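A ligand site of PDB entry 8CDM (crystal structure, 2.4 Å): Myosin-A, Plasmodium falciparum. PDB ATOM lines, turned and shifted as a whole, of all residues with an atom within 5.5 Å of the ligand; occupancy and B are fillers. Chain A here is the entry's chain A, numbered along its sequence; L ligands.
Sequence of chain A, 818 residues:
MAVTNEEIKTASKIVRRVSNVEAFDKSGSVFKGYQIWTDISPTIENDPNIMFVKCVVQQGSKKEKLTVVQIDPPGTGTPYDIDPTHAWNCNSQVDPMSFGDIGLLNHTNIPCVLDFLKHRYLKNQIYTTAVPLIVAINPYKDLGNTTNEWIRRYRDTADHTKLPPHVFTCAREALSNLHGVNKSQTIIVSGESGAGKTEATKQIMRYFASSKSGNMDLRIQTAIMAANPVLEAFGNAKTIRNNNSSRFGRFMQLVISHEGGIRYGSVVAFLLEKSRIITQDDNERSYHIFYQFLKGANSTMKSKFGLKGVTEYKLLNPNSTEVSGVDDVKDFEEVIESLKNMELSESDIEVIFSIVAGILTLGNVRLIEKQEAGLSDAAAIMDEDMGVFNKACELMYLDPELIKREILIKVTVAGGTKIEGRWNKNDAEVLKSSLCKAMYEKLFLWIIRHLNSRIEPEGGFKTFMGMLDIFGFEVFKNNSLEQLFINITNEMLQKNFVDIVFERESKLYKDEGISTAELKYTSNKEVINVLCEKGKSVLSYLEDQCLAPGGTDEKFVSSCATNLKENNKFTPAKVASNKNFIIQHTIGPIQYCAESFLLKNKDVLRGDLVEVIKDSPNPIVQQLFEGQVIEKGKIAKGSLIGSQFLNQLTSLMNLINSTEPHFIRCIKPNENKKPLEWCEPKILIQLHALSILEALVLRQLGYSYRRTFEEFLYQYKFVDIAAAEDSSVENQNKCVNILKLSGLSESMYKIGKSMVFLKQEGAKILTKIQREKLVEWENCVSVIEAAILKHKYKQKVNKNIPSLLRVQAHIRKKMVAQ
A nitrogen (N2) of the ligand lies close to the backbone carbonyl oxygen (O) of Phe 248, 3.2 Å away. N3 of the ligand lies within hydrogen-bond range of N of Phe 471 (3.1 Å).
O of Phe 485 lies within hydrogen-bond range of OG1 of Thr 489, 3.0 Å away. O of Phe 471 sits at hydrogen-bond distance from ND2 of Asn 490, at 3.1 Å. O of Phe 270 is in hydrogen-bond range of N of Gly 249 (2.8 Å). NH1 of Arg 247 is in salt-bridge range of OE1 of Glu 273 (3.1 Å). OE1 of Glu 482 is in salt-bridge range of NZ of Lys 600 (2.8 Å). O of Ile 486 sits at hydrogen-bond distance from ND2 of Asn 490 (2.9 Å).
Ser 246 touches the ligand. Arg 247 touches the ligand. N of Gly 249 touches C16 of the ligand (3.5 Å). Phe 270 touches the ligand. Leu 271 touches the ligand (O to C2, 3.3 Å). Glu 273 touches the ligand (CB to C15, 3.7 Å). Ile 470 touches the ligand (CA to N3, 3.5 Å). Glu 482 touches the ligand (CA to C13, 3.6 Å). Phe 485 touches the ligand. Ile 486 touches the ligand. OG1 of Thr 489 touches C6 of the ligand, at 3.4 Å. CZ of Phe 645 touches C6 of the ligand (3.9 Å). Hydrophobic or aromatic side chains that line the ligand: Phe 270, Leu 271, Ile 470, Phe 471, Phe 485 and Phe 645. 14 residues have an atom within 4 Å of the ligand: Ser 246, Arg 247, Phe 248, Gly 249, Phe 270, Leu 271, Glu 273, Ile 470, Phe 471, Glu 482, Phe 485, Ile 486, Thr 489 and Phe 645.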
ATOM      1  N   SER A 246      21.782  10.989 -24.967  1.00  0.00           N
ATOM      2  CA  SER A 246      21.947  12.300 -24.350  1.00  0.00           C
ATOM      3  C   SER A 246      22.974  13.116 -25.108  1.00  0.00           C
ATOM      4  O   SER A 246      24.134  12.709 -25.221  1.00  0.00           O
ATOM      5  CB  SER A 246      22.394  12.156 -22.906  1.00  0.00           C
ATOM      6  OG  SER A 246      21.297  11.858 -22.122  1.00  0.00           O
ATOM      7  N   ARG A 247      22.557  14.289 -25.580  1.00  0.00           N
ATOM      8  CA  ARG A 247      23.375  15.198 -26.386  1.00  0.00           C
ATOM      9  C   ARG A 247      23.854  16.408 -25.598  1.00  0.00           C
ATOM     10  O   ARG A 247      24.041  17.475 -26.178  1.00  0.00           O
ATOM     11  CB  ARG A 247      22.566  15.640 -27.586  1.00  0.00           C
ATOM     12  CG  ARG A 247      22.054  14.495 -28.327  1.00  0.00           C
ATOM     13  CD  ARG A 247      23.024  14.227 -29.412  1.00  0.00           C
ATOM     14  NE  ARG A 247      23.661  12.957 -29.180  1.00  0.00           N
ATOM     15  CZ  ARG A 247      24.721  12.529 -29.835  1.00  0.00           C
ATOM     16  NH1 ARG A 247      25.295  13.219 -30.809  1.00  0.00           N
ATOM     17  NH2 ARG A 247      25.234  11.371 -29.499  1.00  0.00           N
ATOM     18  N   PHE A 248      23.993  16.268 -24.286  1.00  0.00           N
ATOM     19  CA  PHE A 248      24.517  17.289 -23.387  1.00  0.00           C
ATOM     20  C   PHE A 248      25.144  16.563 -22.214  1.00  0.00           C
ATOM     21  O   PHE A 248      24.812  15.424 -21.934  1.00  0.00           O
ATOM     22  CB  PHE A 248      23.421  18.240 -22.886  1.00  0.00           C
ATOM     23  CG  PHE A 248      22.351  17.538 -22.092  1.00  0.00           C
ATOM     24  CD1 PHE A 248      21.344  16.826 -22.744  1.00  0.00           C
ATOM     25  CD2 PHE A 248      22.360  17.553 -20.704  1.00  0.00           C
ATOM     26  CE1 PHE A 248      20.383  16.165 -22.040  1.00  0.00           C
ATOM     27  CE2 PHE A 248      21.398  16.895 -19.991  1.00  0.00           C
ATOM     28  CZ  PHE A 248      20.403  16.207 -20.651  1.00  0.00           C
ATOM     29  N   GLY A 249      26.052  17.234 -21.514  1.00  0.00           N
ATOM     30  CA  GLY A 249      26.598  16.699 -20.284  1.00  0.00           C
ATOM     31  C   GLY A 249      25.745  17.147 -19.106  1.00  0.00           C
ATOM     32  O   GLY A 249      25.269  18.277 -19.061  1.00  0.00           O
ATOM     33  N   PHE A 270      25.654  21.088 -19.903  1.00  0.00           N
ATOM     34  CA  PHE A 270      26.652  21.782 -20.702  1.00  0.00           C
ATOM     35  C   PHE A 270      26.865  21.110 -22.067  1.00  0.00           C
ATOM     36  O   PHE A 270      26.558  19.935 -22.267  1.00  0.00           O
ATOM     37  CB  PHE A 270      27.986  21.908 -19.936  1.00  0.00           C
ATOM     38  CG  PHE A 270      28.500  20.600 -19.411  1.00  0.00           C
ATOM     39  CD1 PHE A 270      28.076  20.103 -18.184  1.00  0.00           C
ATOM     40  CD2 PHE A 270      29.419  19.860 -20.144  1.00  0.00           C
ATOM     41  CE1 PHE A 270      28.562  18.893 -17.700  1.00  0.00           C
ATOM     42  CE2 PHE A 270      29.909  18.638 -19.666  1.00  0.00           C
ATOM     43  CZ  PHE A 270      29.478  18.159 -18.446  1.00  0.00           C
ATOM     44  N   LEU A 271      27.347  21.899 -23.025  1.00  0.00           N
ATOM     45  CA  LEU A 271      27.666  21.455 -24.392  1.00  0.00           C
ATOM     46  C   LEU A 271      26.478  20.737 -25.051  1.00  0.00           C
ATOM     47  O   LEU A 271      26.586  19.601 -25.490  1.00  0.00           O
ATOM     48  CB  LEU A 271      28.917  20.570 -24.405  1.00  0.00           C
ATOM     49  CG  LEU A 271      30.186  21.324 -24.033  1.00  0.00           C
ATOM     50  CD1 LEU A 271      31.419  20.473 -24.191  1.00  0.00           C
ATOM     51  CD2 LEU A 271      30.294  22.598 -24.865  1.00  0.00           C
ATOM     52  N   LEU A 272      25.348  21.436 -25.124  1.00  0.00           N
ATOM     53  CA  LEU A 272      24.235  20.901 -25.911  1.00  0.00           C
ATOM     54  C   LEU A 272      24.627  20.897 -27.378  1.00  0.00           C
ATOM     55  O   LEU A 272      25.265  21.831 -27.878  1.00  0.00           O
ATOM     56  CB  LEU A 272      22.967  21.739 -25.698  1.00  0.00           C
ATOM     57  CG  LEU A 272      21.709  21.331 -26.485  1.00  0.00           C
ATOM     58  CD1 LEU A 272      21.217  19.920 -26.095  1.00  0.00           C
ATOM     59  CD2 LEU A 272      20.587  22.315 -26.313  1.00  0.00           C
ATOM     60  N   GLU A 273      24.285  19.817 -28.072  1.00  0.00           N
ATOM     61  CA  GLU A 273      24.566  19.657 -29.501  1.00  0.00           C
ATOM     62  C   GLU A 273      23.574  20.508 -30.287  1.00  0.00           C
ATOM     63  O   GLU A 273      22.573  20.017 -30.809  1.00  0.00           O
ATOM     64  CB  GLU A 273      24.501  18.194 -29.917  1.00  0.00           C
ATOM     65  CG  GLU A 273      25.263  17.919 -31.173  1.00  0.00           C
ATOM     66  CD  GLU A 273      25.110  16.504 -31.693  1.00  0.00           C
ATOM     67  OE1 GLU A 273      24.024  15.911 -31.570  1.00  0.00           O
ATOM     68  OE2 GLU A 273      26.090  15.985 -32.268  1.00  0.00           O
ATOM     69  N   ASP A 469      27.096  12.535 -15.567  1.00  0.00           N
ATOM     70  CA  ASP A 469      26.707  11.568 -16.602  1.00  0.00           C
ATOM     71  C   ASP A 469      27.218  12.046 -17.953  1.00  0.00           C
ATOM     72  O   ASP A 469      26.629  12.957 -18.547  1.00  0.00           O
ATOM     73  CB  ASP A 469      25.185  11.397 -16.627  1.00  0.00           C
ATOM     74  CG  ASP A 469      24.717  10.408 -17.694  1.00  0.00           C
ATOM     75  OD1 ASP A 469      25.284  10.349 -18.807  1.00  0.00           O
ATOM     76  OD2 ASP A 469      23.732   9.682 -17.409  1.00  0.00           O
ATOM     77  N   ILE A 470      28.276  11.414 -18.486  1.00  0.00           N
ATOM     78  CA  ILE A 470      29.007  11.954 -19.632  1.00  0.00           C
ATOM     79  C   ILE A 470      29.522  10.825 -20.537  1.00  0.00           C
ATOM     80  O   ILE A 470      29.668   9.683 -20.117  1.00  0.00           O
ATOM     81  CB  ILE A 470      30.189  12.834 -19.156  1.00  0.00           C
ATOM     82  CG1 ILE A 470      30.961  12.117 -18.046  1.00  0.00           C
ATOM     83  CG2 ILE A 470      29.704  14.180 -18.635  1.00  0.00           C
ATOM     84  CD1 ILE A 470      32.441  12.332 -18.119  1.00  0.00           C
ATOM     85  N   PHE A 471      29.812  11.166 -21.783  1.00  0.00           N
ATOM     86  CA  PHE A 471      30.642  10.311 -22.620  1.00  0.00           C
ATOM     87  C   PHE A 471      31.982  10.081 -21.930  1.00  0.00           C
ATOM     88  O   PHE A 471      32.521  10.979 -21.273  1.00  0.00           O
ATOM     89  CB  PHE A 471      30.898  10.979 -23.965  1.00  0.00           C
ATOM     90  CG  PHE A 471      29.763  10.899 -24.943  1.00  0.00           C
ATOM     91  CD1 PHE A 471      29.372   9.686 -25.472  1.00  0.00           C
ATOM     92  CD2 PHE A 471      29.119  12.054 -25.379  1.00  0.00           C
ATOM     93  CE1 PHE A 471      28.340   9.621 -26.402  1.00  0.00           C
ATOM     94  CE2 PHE A 471      28.086  11.993 -26.300  1.00  0.00           C
ATOM     95  CZ  PHE A 471      27.703  10.787 -26.820  1.00  0.00           C
ATOM     96  N   LEU A 481      36.038  18.898 -32.988  1.00  0.00           N
ATOM     97  CA  LEU A 481      36.089  19.702 -31.776  1.00  0.00           C
ATOM     98  C   LEU A 481      35.227  19.106 -30.665  1.00  0.00           C
ATOM     99  O   LEU A 481      35.589  19.186 -29.481  1.00  0.00           O
ATOM    100  CB  LEU A 481      35.627  21.119 -32.100  1.00  0.00           C
ATOM    101  CG  LEU A 481      35.796  22.113 -30.960  1.00  0.00           C
ATOM    102  CD1 LEU A 481      37.271  22.272 -30.623  1.00  0.00           C
ATOM    103  CD2 LEU A 481      35.130  23.441 -31.325  1.00  0.00           C
ATOM    104  N   GLU A 482      34.088  18.519 -31.014  1.00  0.00           N
ATOM    105  CA  GLU A 482      33.238  17.939 -29.984  1.00  0.00           C
ATOM    106  C   GLU A 482      33.959  16.813 -29.259  1.00  0.00           C
ATOM    107  O   GLU A 482      33.844  16.684 -28.034  1.00  0.00           O
ATOM    108  CB  GLU A 482      31.933  17.421 -30.582  1.00  0.00           C
ATOM    109  CG  GLU A 482      31.075  18.497 -31.216  1.00  0.00           C
ATOM    110  CD  GLU A 482      31.256  18.592 -32.712  1.00  0.00           C
ATOM    111  OE1 GLU A 482      32.387  18.413 -33.209  1.00  0.00           O
ATOM    112  OE2 GLU A 482      30.260  18.849 -33.418  1.00  0.00           O
ATOM    113  N   GLN A 483      34.730  16.012 -29.995  1.00  0.00           N
ATOM    114  CA  GLN A 483      35.461  14.931 -29.362  1.00  0.00           C
ATOM    115  C   GLN A 483      36.619  15.465 -28.538  1.00  0.00           C
ATOM    116  O   GLN A 483      36.942  14.907 -27.475  1.00  0.00           O
ATOM    117  CB  GLN A 483      35.940  13.935 -30.410  1.00  0.00           C
ATOM    118  CG  GLN A 483      34.852  13.005 -30.899  1.00  0.00           C
ATOM    119  CD  GLN A 483      33.937  13.660 -31.914  1.00  0.00           C
ATOM    120  OE1 GLN A 483      34.363  14.503 -32.694  1.00  0.00           O
ATOM    121  NE2 GLN A 483      32.677  13.284 -31.905  1.00  0.00           N
ATOM    122  N   PHE A 485      36.685  18.297 -26.768  1.00  0.00           N
ATOM    123  CA  PHE A 485      36.157  18.749 -25.481  1.00  0.00           C
ATOM    124  C   PHE A 485      35.833  17.570 -24.579  1.00  0.00           C
ATOM    125  O   PHE A 485      36.187  17.556 -23.391  1.00  0.00           O
ATOM    126  CB  PHE A 485      34.901  19.595 -25.690  1.00  0.00           C
ATOM    127  CG  PHE A 485      35.156  20.924 -26.344  1.00  0.00           C
ATOM    128  CD1 PHE A 485      36.424  21.471 -26.365  1.00  0.00           C
ATOM    129  CD2 PHE A 485      34.115  21.615 -26.944  1.00  0.00           C
ATOM    130  CE1 PHE A 485      36.657  22.697 -26.970  1.00  0.00           C
ATOM    131  CE2 PHE A 485      34.348  22.841 -27.549  1.00  0.00           C
ATOM    132  CZ  PHE A 485      35.616  23.388 -27.571  1.00  0.00           C
ATOM    133  N   ILE A 486      35.158  16.562 -25.122  1.00  0.00           N
ATOM    134  CA  ILE A 486      34.910  15.337 -24.368  1.00  0.00           C
ATOM    135  C   ILE A 486      36.217  14.754 -23.846  1.00  0.00           C
ATOM    136  O   ILE A 486      36.314  14.378 -22.662  1.00  0.00           O
ATOM    137  CB  ILE A 486      34.141  14.341 -25.250  1.00  0.00           C
ATOM    138  CG1 ILE A 486      32.786  14.953 -25.637  1.00  0.00           C
ATOM    139  CG2 ILE A 486      34.006  12.985 -24.529  1.00  0.00           C
ATOM    140  CD1 ILE A 486      31.893  14.041 -26.425  1.00  0.00           C
ATOM    141  N   THR A 489      37.798  16.607 -20.998  1.00  0.00           N
ATOM    142  CA  THR A 489      37.065  16.332 -19.750  1.00  0.00           C
ATOM    143  C   THR A 489      37.542  15.047 -19.109  1.00  0.00           C
ATOM    144  O   THR A 489      37.807  14.989 -17.913  1.00  0.00           O
ATOM    145  CB  THR A 489      35.557  16.268 -19.998  1.00  0.00           C
ATOM    146  OG1 THR A 489      35.106  17.487 -20.600  1.00  0.00           O
ATOM    147  CG2 THR A 489      34.782  16.078 -18.703  1.00  0.00           C
ATOM    148  N   ASN A 490      37.678  13.996 -19.914  1.00  0.00           N
ATOM    149  CA  ASN A 490      38.052  12.688 -19.393  1.00  0.00           C
ATOM    150  C   ASN A 490      39.526  12.604 -19.026  1.00  0.00           C
ATOM    151  O   ASN A 490      39.898  11.685 -18.302  1.00  0.00           O
ATOM    152  CB  ASN A 490      37.685  11.611 -20.404  1.00  0.00           C
ATOM    153  CG  ASN A 490      36.217  11.305 -20.391  1.00  0.00           C
ATOM    154  OD1 ASN A 490      35.768  10.463 -19.614  1.00  0.00           O
ATOM    155  ND2 ASN A 490      35.452  11.974 -21.244  1.00  0.00           N
ATOM    156  N   LYS A 600      32.992  25.779 -35.648  1.00  0.00           N
ATOM    157  CA  LYS A 600      32.321  25.163 -34.519  1.00  0.00           C
ATOM    158  C   LYS A 600      32.526  25.964 -33.245  1.00  0.00           C
ATOM    159  O   LYS A 600      31.582  26.212 -32.496  1.00  0.00           O
ATOM    160  CB  LYS A 600      32.803  23.734 -34.350  1.00  0.00           C
ATOM    161  CG  LYS A 600      32.185  22.829 -35.402  1.00  0.00           C
ATOM    162  CD  LYS A 600      32.710  21.414 -35.374  1.00  0.00           C
ATOM    163  CE  LYS A 600      31.614  20.475 -35.849  1.00  0.00           C
ATOM    164  NZ  LYS A 600      32.066  19.073 -35.910  1.00  0.00           N
ATOM    165  N   ILE A 641      32.705  28.858 -27.644  1.00  0.00           N
ATOM    166  CA  ILE A 641      32.310  27.678 -26.891  1.00  0.00           C
ATOM    167  C   ILE A 641      33.485  27.132 -26.106  1.00  0.00           C
ATOM    168  O   ILE A 641      33.348  26.722 -24.946  1.00  0.00           O
ATOM    169  CB  ILE A 641      31.715  26.615 -27.846  1.00  0.00           C
ATOM    170  CG1 ILE A 641      30.503  27.177 -28.587  1.00  0.00           C
ATOM    171  CG2 ILE A 641      31.315  25.338 -27.099  1.00  0.00           C
ATOM    172  CD1 ILE A 641      29.980  26.279 -29.632  1.00  0.00           C
ATOM    173  N   PHE A 645      33.708  26.840 -22.125  1.00  0.00           N
ATOM    174  CA  PHE A 645      33.667  25.497 -21.593  1.00  0.00           C
ATOM    175  C   PHE A 645      34.803  25.241 -20.613  1.00  0.00           C
ATOM    176  O   PHE A 645      34.605  24.584 -19.590  1.00  0.00           O
ATOM    177  CB  PHE A 645      33.713  24.452 -22.701  1.00  0.00           C
ATOM    178  CG  PHE A 645      33.708  23.045 -22.162  1.00  0.00           C
ATOM    179  CD1 PHE A 645      32.649  22.591 -21.398  1.00  0.00           C
ATOM    180  CD2 PHE A 645      34.775  22.195 -22.403  1.00  0.00           C
ATOM    181  CE1 PHE A 645      32.646  21.316 -20.878  1.00  0.00           C
ATOM    182  CE2 PHE A 645      34.777  20.909 -21.889  1.00  0.00           C
ATOM    183  CZ  PHE A 645      33.711  20.471 -21.133  1.00  0.00           C
HETATM  184  C1  LIG L   1      28.091  15.839 -28.527  1.00  0.00           C
HETATM  185  N1  LIG L   1      28.383  16.143 -26.121  1.00  0.00           N
HETATM  186  C2  LIG L   1      27.857  16.674 -24.843  1.00  0.00           C
HETATM  187  C3  LIG L   1      26.781  14.465 -23.956  1.00  0.00           C
HETATM  188  C4  LIG L   1      31.124  14.943 -21.800  1.00  0.00           C
HETATM  189  C5  LIG L   1      32.268  15.786 -21.562  1.00  0.00           C
HETATM  190  C6  LIG L   1      32.162  17.058 -22.147  1.00  0.00           C
HETATM  191  C7  LIG L   1      31.190  21.781 -29.520  1.00  0.00           C
HETATM  192  C8  LIG L   1      30.506  20.118 -28.059  1.00  0.00           C
HETATM  193  C9  LIG L   1      29.171  20.230 -28.465  1.00  0.00           C
HETATM  194  C10 LIG L   1      28.296  19.156 -28.227  1.00  0.00           C
HETATM  195  C11 LIG L   1      28.767  17.997 -27.614  1.00  0.00           C
HETATM  196  C12 LIG L   1      30.103  17.885 -27.208  1.00  0.00           C
HETATM  197  C13 LIG L   1      30.970  18.951 -27.433  1.00  0.00           C
HETATM  198  C14 LIG L   1      27.839  16.789 -27.340  1.00  0.00           C
HETATM  199  C15 LIG L   1      26.691  15.949 -27.914  1.00  0.00           C
HETATM  200  C16 LIG L   1      27.818  15.421 -23.946  1.00  0.00           C
HETATM  201  C17 LIG L   1      28.784  14.933 -23.024  1.00  0.00           C
HETATM  202  C18 LIG L   1      30.118  15.549 -22.601  1.00  0.00           C
HETATM  203  N2  LIG L   1      27.147  13.550 -23.083  1.00  0.00           N
HETATM  204  N3  LIG L   1      28.324  13.812 -22.528  1.00  0.00           N
HETATM  205  O1  LIG L   1      31.384  21.186 -28.262  1.00  0.00           O
HETATM  206  S1  LIG L   1      30.667  17.092 -22.983  1.00  0.00           S
